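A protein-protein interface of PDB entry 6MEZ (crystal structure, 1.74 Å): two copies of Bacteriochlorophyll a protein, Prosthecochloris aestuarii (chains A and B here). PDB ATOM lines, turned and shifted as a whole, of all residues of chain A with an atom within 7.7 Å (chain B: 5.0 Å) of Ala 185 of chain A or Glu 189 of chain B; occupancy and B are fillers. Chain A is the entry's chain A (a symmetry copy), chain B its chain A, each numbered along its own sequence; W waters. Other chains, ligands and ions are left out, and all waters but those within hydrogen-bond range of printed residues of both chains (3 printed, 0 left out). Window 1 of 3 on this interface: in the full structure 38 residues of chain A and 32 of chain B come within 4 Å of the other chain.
The backbone NH of Phe 184 of chain A lies within hydrogen-bond range of the backbone carbonyl oxygen of Phe 179 of chain A.
Phe 184 of chain A touches Asn 188 of chain B.
Phe 184 of chain A touches Gly 191 of chain B.
Ala 185 of chain A touches Asn 188 of chain B.
Ala 185 of chain A touches Glu 189 of chain B (CB to O, 3.6 Å).
Asn 188 of chain B touches Asn 188 of chain A (OD1 to CB, 3.8 Å).
Of the printed residues of chain B, Phe 184 of chain A touches Asn 188 and Gly 191.
Printed residues of chain B within 4 Å of Ala 185 of chain A: Asn 188 and Glu 189.
Ala 186 of chain A touches none of the printed residues of chain B.
Of the printed residues of chain B, Asn 188 of chain A touches Asn 188.
His 291 of chain A touches none of the printed residues of chain B.
Printed residues of chain A within 4 Å of Asn 188 of chain B: Phe 184, Ala 185 and Asn 188.
Of the printed residues of chain A, Glu 189 of chain B touches Ala 185 (3.6 Å).
Of the printed residues of chain A, Gly 191 of chain B touches Phe 184.
The nearest printed residue of chain A that does not touch Glu 189 of chain B is Glu 189 of chain A (5.1 Å).
The nearest printed residue of chain A that does not touch Asn 188 of chain B is Ala 186 of chain A (5.7 Å).
Hydrophobic or aromatic side chains of chain A that line the printed part of chain B: Phe 184 and Ala 185.
Among the printed residues, no Asp or Glu carboxylate lies within 4 Å of a Lys or Arg side-chain nitrogen of the other chain.
Ala 185 of chain A touches Asn 188 of chain B, but with the chains exchanged Asn 188 of chain A does not touch Ala 185 of chain B (8.0 Å).
Ala 185 of chain A touches Glu 189 of chain B, but with the chains exchanged Glu 189 of chain A does not touch Ala 185 of chain B (8.6 Å).
Asn 188 of chain A touches its own counterpart, Asn 188 of chain B.
Positions printed for both chains: 185, 186, 187, 188, 189, 190, 191 and 294.
Water W3 lies within hydrogen-bond range of the backbone carbonyl oxygen of Phe 184 of chain A (2.6 Å), the side-chain amide oxygen of Asn 188 of chain B (2.9 Å) and the backbone NH of Asn 188 of chain A (3.0 Å).
Water W2 lies within hydrogen-bond range of O of Gly 181 of chain A (2.7 Å), N of Ala 185 of chain A (3.0 Å) and N of Gly 191 of chain B (3.4 Å).
Water W1 bridges OE1 of Glu 189 of chain B (3.1 Å) and OE1 of Glu 189 of chain A (3.1 Å).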
ATOM      1  N   PHE A 179      18.316  -9.923 -24.999  1.00  0.00           N
ATOM      2  CA  PHE A 179      18.048 -11.104 -24.186  1.00  0.00           C
ATOM      3  C   PHE A 179      18.382 -12.361 -24.976  1.00  0.00           C
ATOM      4  O   PHE A 179      17.533 -13.142 -25.409  1.00  0.00           O
ATOM      5  CB  PHE A 179      16.616 -11.049 -23.660  1.00  0.00           C
ATOM      6  CG  PHE A 179      16.423  -9.924 -22.672  1.00  0.00           C
ATOM      7  CD1 PHE A 179      16.946 -10.026 -21.391  1.00  0.00           C
ATOM      8  CD2 PHE A 179      15.800  -8.737 -23.041  1.00  0.00           C
ATOM      9  CE1 PHE A 179      16.814  -8.985 -20.479  1.00  0.00           C
ATOM     10  CE2 PHE A 179      15.674  -7.690 -22.136  1.00  0.00           C
ATOM     11  CZ  PHE A 179      16.175  -7.820 -20.850  1.00  0.00           C
ATOM     12  N   ILE A 180      19.681 -12.524 -25.132  1.00  0.00           N
ATOM     13  CA  ILE A 180      20.271 -13.574 -25.940  1.00  0.00           C
ATOM     14  C   ILE A 180      19.873 -14.977 -25.500  1.00  0.00           C
ATOM     15  O   ILE A 180      19.699 -15.250 -24.310  1.00  0.00           O
ATOM     16  CB  ILE A 180      21.817 -13.410 -25.931  1.00  0.00           C
ATOM     17  CG1 ILE A 180      22.487 -14.376 -26.910  1.00  0.00           C
ATOM     18  CG2 ILE A 180      22.380 -13.551 -24.508  1.00  0.00           C
ATOM     19  CD1 ILE A 180      23.974 -14.084 -27.099  1.00  0.00           C
ATOM     20  N   GLY A 181      19.727 -15.862 -26.480  1.00  0.00           N
ATOM     21  CA  GLY A 181      19.481 -17.271 -26.206  1.00  0.00           C
ATOM     22  C   GLY A 181      18.212 -17.458 -25.387  1.00  0.00           C
ATOM     23  O   GLY A 181      17.183 -16.833 -25.669  1.00  0.00           O
ATOM     24  N   PRO A 182      18.277 -18.314 -24.354  1.00  0.00           N
ATOM     25  CA  PRO A 182      17.064 -18.626 -23.586  1.00  0.00           C
ATOM     26  C   PRO A 182      16.628 -17.505 -22.648  1.00  0.00           C
ATOM     27  O   PRO A 182      15.586 -17.626 -22.006  1.00  0.00           O
ATOM     28  CB  PRO A 182      17.472 -19.861 -22.789  1.00  0.00           C
ATOM     29  CG  PRO A 182      18.933 -19.679 -22.586  1.00  0.00           C
ATOM     30  CD  PRO A 182      19.442 -19.074 -23.871  1.00  0.00           C
ATOM     31  N   ALA A 183      17.388 -16.411 -22.586  1.00  0.00           N
ATOM     32  CA  ALA A 183      16.970 -15.290 -21.743  1.00  0.00           C
ATOM     33  C   ALA A 183      15.647 -14.702 -22.236  1.00  0.00           C
ATOM     34  O   ALA A 183      14.822 -14.272 -21.440  1.00  0.00           O
ATOM     35  CB  ALA A 183      18.065 -14.183 -21.705  1.00  0.00           C
ATOM     36  N   PHE A 184      15.419 -14.689 -23.544  1.00  0.00           N
ATOM     37  CA  PHE A 184      14.188 -14.067 -24.041  1.00  0.00           C
ATOM     38  C   PHE A 184      12.927 -14.790 -23.529  1.00  0.00           C
ATOM     39  O   PHE A 184      11.974 -14.149 -23.059  1.00  0.00           O
ATOM     40  CB  PHE A 184      14.200 -14.038 -25.573  1.00  0.00           C
ATOM     41  CG  PHE A 184      13.105 -13.195 -26.165  1.00  0.00           C
ATOM     42  CD1 PHE A 184      11.857 -13.738 -26.408  1.00  0.00           C
ATOM     43  CD2 PHE A 184      13.321 -11.860 -26.456  1.00  0.00           C
ATOM     44  CE1 PHE A 184      10.840 -12.970 -26.951  1.00  0.00           C
ATOM     45  CE2 PHE A 184      12.299 -11.081 -27.003  1.00  0.00           C
ATOM     46  CZ  PHE A 184      11.067 -11.642 -27.250  1.00  0.00           C
ATOM     47  N   ALA A 185      12.910 -16.120 -23.626  1.00  0.00           N
ATOM     48  CA  ALA A 185      11.762 -16.899 -23.165  1.00  0.00           C
ATOM     49  C   ALA A 185      11.507 -16.720 -21.667  1.00  0.00           C
ATOM     50  O   ALA A 185      10.353 -16.789 -21.218  1.00  0.00           O
ATOM     51  CB  ALA A 185      11.959 -18.400 -23.481  1.00  0.00           C
ATOM     52  N   ALA A 186      12.568 -16.480 -20.902  1.00  0.00           N
ATOM     53  CA  ALA A 186      12.418 -16.406 -19.450  1.00  0.00           C
ATOM     54  C   ALA A 186      11.675 -15.156 -19.012  1.00  0.00           C
ATOM     55  O   ALA A 186      11.152 -15.132 -17.901  1.00  0.00           O
ATOM     56  CB  ALA A 186      13.784 -16.483 -18.743  1.00  0.00           C
ATOM     57  N   ILE A 187      11.623 -14.131 -19.863  1.00  0.00           N
ATOM     58  CA  ILE A 187      10.911 -12.891 -19.511  1.00  0.00           C
ATOM     59  C   ILE A 187       9.435 -13.193 -19.226  1.00  0.00           C
ATOM     60  O   ILE A 187       8.937 -12.938 -18.130  1.00  0.00           O
ATOM     61  CB  ILE A 187      11.030 -11.824 -20.621  1.00  0.00           C
ATOM     62  CG1 ILE A 187      12.495 -11.433 -20.832  1.00  0.00           C
ATOM     63  CG2 ILE A 187      10.212 -10.590 -20.274  1.00  0.00           C
ATOM     64  CD1 ILE A 187      12.738 -10.662 -22.156  1.00  0.00           C
ATOM     65  N   ASN A 188       8.721 -13.771 -20.159  1.00  0.00           N
ATOM     66  CA  ASN A 188       7.318 -14.082 -19.937  1.00  0.00           C
ATOM     67  C   ASN A 188       7.119 -15.097 -18.806  1.00  0.00           C
ATOM     68  O   ASN A 188       6.164 -15.057 -18.106  1.00  0.00           O
ATOM     69  CB  ASN A 188       6.681 -14.590 -21.219  1.00  0.00           C
ATOM     70  CG  ASN A 188       5.172 -14.418 -21.243  1.00  0.00           C
ATOM     71  OD1 ASN A 188       4.485 -15.328 -21.100  1.00  0.00           O
ATOM     72  ND2 ASN A 188       4.715 -13.231 -21.509  1.00  0.00           N
ATOM     73  N   GLU A 189       8.053 -16.016 -18.692  1.00  0.00           N
ATOM     74  CA  GLU A 189       7.912 -17.080 -17.683  1.00  0.00           C
ATOM     75  C   GLU A 189       7.731 -16.512 -16.282  1.00  0.00           C
ATOM     76  O   GLU A 189       7.014 -17.088 -15.463  1.00  0.00           O
ATOM     77  CB  GLU A 189       9.132 -18.018 -17.695  1.00  0.00           C
ATOM     78  CG  GLU A 189       8.986 -19.270 -16.816  1.00  0.00           C
ATOM     79  CD  GLU A 189       8.448 -20.467 -17.587  1.00  0.00           C
ATOM     80  OE1 GLU A 189       8.046 -20.297 -18.761  1.00  0.00           O
ATOM     81  OE2 GLU A 189       8.437 -21.583 -17.022  1.00  0.00           O
ATOM     82  N   GLY A 190       8.387 -15.385 -16.006  1.00  0.00           N
ATOM     83  CA  GLY A 190       8.293 -14.741 -14.707  1.00  0.00           C
ATOM     84  C   GLY A 190       7.226 -13.661 -14.628  1.00  0.00           C
ATOM     85  O   GLY A 190       7.204 -12.893 -13.673  1.00  0.00           O
ATOM     86  N   GLY A 191       6.341 -13.593 -15.619  1.00  0.00           N
ATOM     87  CA  GLY A 191       5.305 -12.569 -15.649  1.00  0.00           C
ATOM     88  C   GLY A 191       5.889 -11.175 -15.806  1.00  0.00           C
ATOM     89  O   GLY A 191       5.338 -10.207 -15.274  1.00  0.00           O
ATOM     90  N   HIS A 291      12.869 -19.149 -12.715  1.00  0.00           N
ATOM     91  CA  HIS A 291      13.882 -19.259 -13.737  1.00  0.00           C
ATOM     92  C   HIS A 291      14.677 -20.564 -13.688  1.00  0.00           C
ATOM     93  O   HIS A 291      14.894 -21.168 -14.667  1.00  0.00           O
ATOM     94  CB  HIS A 291      14.831 -18.061 -13.724  1.00  0.00           C
ATOM     95  CG  HIS A 291      14.193 -16.812 -14.210  1.00  0.00           C
ATOM     96  ND1 HIS A 291      14.877 -15.653 -14.420  1.00  0.00           N
ATOM     97  CD2 HIS A 291      12.929 -16.571 -14.594  1.00  0.00           C
ATOM     98  CE1 HIS A 291      14.061 -14.734 -14.863  1.00  0.00           C
ATOM     99  NE2 HIS A 291      12.870 -15.265 -14.992  1.00  0.00           N
ATOM    100  N   MET A 294      13.217 -23.557 -15.146  1.00  0.00           N
ATOM    101  CA  MET A 294      13.269 -23.821 -16.568  1.00  0.00           C
ATOM    102  C   MET A 294      14.346 -24.851 -16.951  1.00  0.00           C
ATOM    103  O   MET A 294      14.351 -25.342 -18.031  1.00  0.00           O
ATOM    104  CB  MET A 294      13.485 -22.523 -17.320  1.00  0.00           C
ATOM    105  CG  MET A 294      12.367 -21.540 -17.118  1.00  0.00           C
ATOM    106  SD  MET A 294      12.549 -19.998 -18.029  1.00  0.00           S
ATOM    107  CE  MET A 294      12.221 -20.508 -19.675  1.00  0.00           C
ATOM    108  N   ALA B 185       2.056 -21.080 -28.518  1.00  0.00           N
ATOM    109  CA  ALA B 185       2.879 -21.029 -27.312  1.00  0.00           C
ATOM    110  C   ALA B 185       4.346 -21.352 -27.600  1.00  0.00           C
ATOM    111  O   ALA B 185       5.244 -20.834 -26.921  1.00  0.00           O
ATOM    112  CB  ALA B 185       2.336 -22.003 -26.240  1.00  0.00           C
ATOM    113  N   ALA B 186       4.590 -22.191 -28.604  1.00  0.00           N
ATOM    114  CA  ALA B 186       5.958 -22.632 -28.870  1.00  0.00           C
ATOM    115  C   ALA B 186       6.821 -21.519 -29.438  1.00  0.00           C
ATOM    116  O   ALA B 186       8.043 -21.613 -29.362  1.00  0.00           O
ATOM    117  CB  ALA B 186       5.979 -23.849 -29.813  1.00  0.00           C
ATOM    118  N   ILE B 187       6.205 -20.476 -29.998  1.00  0.00           N
ATOM    119  CA  ILE B 187       6.976 -19.354 -30.559  1.00  0.00           C
ATOM    120  C   ILE B 187       7.843 -18.713 -29.469  1.00  0.00           C
ATOM    121  O   ILE B 187       9.067 -18.668 -29.580  1.00  0.00           O
ATOM    122  CB  ILE B 187       6.059 -18.292 -31.204  1.00  0.00           C
ATOM    123  CG1 ILE B 187       5.274 -18.899 -32.369  1.00  0.00           C
ATOM    124  CG2 ILE B 187       6.872 -17.104 -31.694  1.00  0.00           C
ATOM    125  CD1 ILE B 187       4.078 -18.022 -32.824  1.00  0.00           C
ATOM    126  N   ASN B 188       7.258 -18.251 -28.394  1.00  0.00           N
ATOM    127  CA  ASN B 188       8.036 -17.636 -27.331  1.00  0.00           C
ATOM    128  C   ASN B 188       9.012 -18.621 -26.678  1.00  0.00           C
ATOM    129  O   ASN B 188      10.059 -18.262 -26.258  1.00  0.00           O
ATOM    130  CB  ASN B 188       7.113 -17.037 -26.281  1.00  0.00           C
ATOM    131  CG  ASN B 188       7.775 -15.942 -25.463  1.00  0.00           C
ATOM    132  OD1 ASN B 188       8.099 -16.146 -24.379  1.00  0.00           O
ATOM    133  ND2 ASN B 188       7.878 -14.769 -26.014  1.00  0.00           N
ATOM    134  N   GLU B 189       8.596 -19.866 -26.595  1.00  0.00           N
ATOM    135  CA  GLU B 189       9.431 -20.873 -25.918  1.00  0.00           C
ATOM    136  C   GLU B 189      10.826 -20.952 -26.526  1.00  0.00           C
ATOM    137  O   GLU B 189      11.802 -21.194 -25.815  1.00  0.00           O
ATOM    138  CB  GLU B 189       8.775 -22.263 -25.972  1.00  0.00           C
ATOM    139  CG  GLU B 189       9.476 -23.335 -25.123  1.00  0.00           C
ATOM    140  CD  GLU B 189       8.886 -23.454 -23.725  1.00  0.00           C
ATOM    141  OE1 GLU B 189       8.037 -22.611 -23.356  1.00  0.00           O
ATOM    142  OE2 GLU B 189       9.264 -24.398 -22.997  1.00  0.00           O
ATOM    143  N   GLY B 190      10.915 -20.757 -27.840  1.00  0.00           N
ATOM    144  CA  GLY B 190      12.189 -20.802 -28.538  1.00  0.00           C
ATOM    145  C   GLY B 190      12.854 -19.445 -28.700  1.00  0.00           C
ATOM    146  O   GLY B 190      13.804 -19.317 -29.464  1.00  0.00           O
ATOM    147  N   GLY B 191      12.368 -18.430 -27.991  1.00  0.00           N
ATOM    148  CA  GLY B 191      12.915 -17.085 -28.108  1.00  0.00           C
ATOM    149  C   GLY B 191      12.682 -16.494 -29.488  1.00  0.00           C
ATOM    150  O   GLY B 191      13.511 -15.726 -29.984  1.00  0.00           O
ATOM    151  N   VAL B 290      14.127 -27.845 -27.753  1.00  0.00           N
ATOM    152  CA  VAL B 290      13.272 -26.947 -27.014  1.00  0.00           C
ATOM    153  C   VAL B 290      11.806 -27.243 -27.250  1.00  0.00           C
ATOM    154  O   VAL B 290      11.060 -27.303 -26.350  1.00  0.00           O
ATOM    155  CB  VAL B 290      13.608 -25.493 -27.311  1.00  0.00           C
ATOM    156  CG1 VAL B 290      12.647 -24.553 -26.659  1.00  0.00           C
ATOM    157  CG2 VAL B 290      15.035 -25.227 -26.930  1.00  0.00           C
ATOM    158  N   MET B 294       8.606 -29.521 -24.892  1.00  0.00           N
ATOM    159  CA  MET B 294       7.285 -29.152 -24.428  1.00  0.00           C
ATOM    160  C   MET B 294       6.350 -30.361 -24.246  1.00  0.00           C
ATOM    161  O   MET B 294       5.329 -30.247 -23.654  1.00  0.00           O
ATOM    162  CB  MET B 294       6.672 -28.147 -25.382  1.00  0.00           C
ATOM    163  CG  MET B 294       7.458 -26.869 -25.465  1.00  0.00           C
ATOM    164  SD  MET B 294       6.746 -25.619 -26.548  1.00  0.00           S
ATOM    165  CE  MET B 294       5.364 -25.074 -25.614  1.00  0.00           C
HETATM  166  O   HOH W   1       6.749 -22.423 -20.568  1.00  0.00           O
HETATM  167  O   HOH W   2      14.616 -17.654 -25.504  1.00  0.00           O
HETATM  168  O   HOH W   3       9.364 -13.870 -23.104  1.00  0.00           O
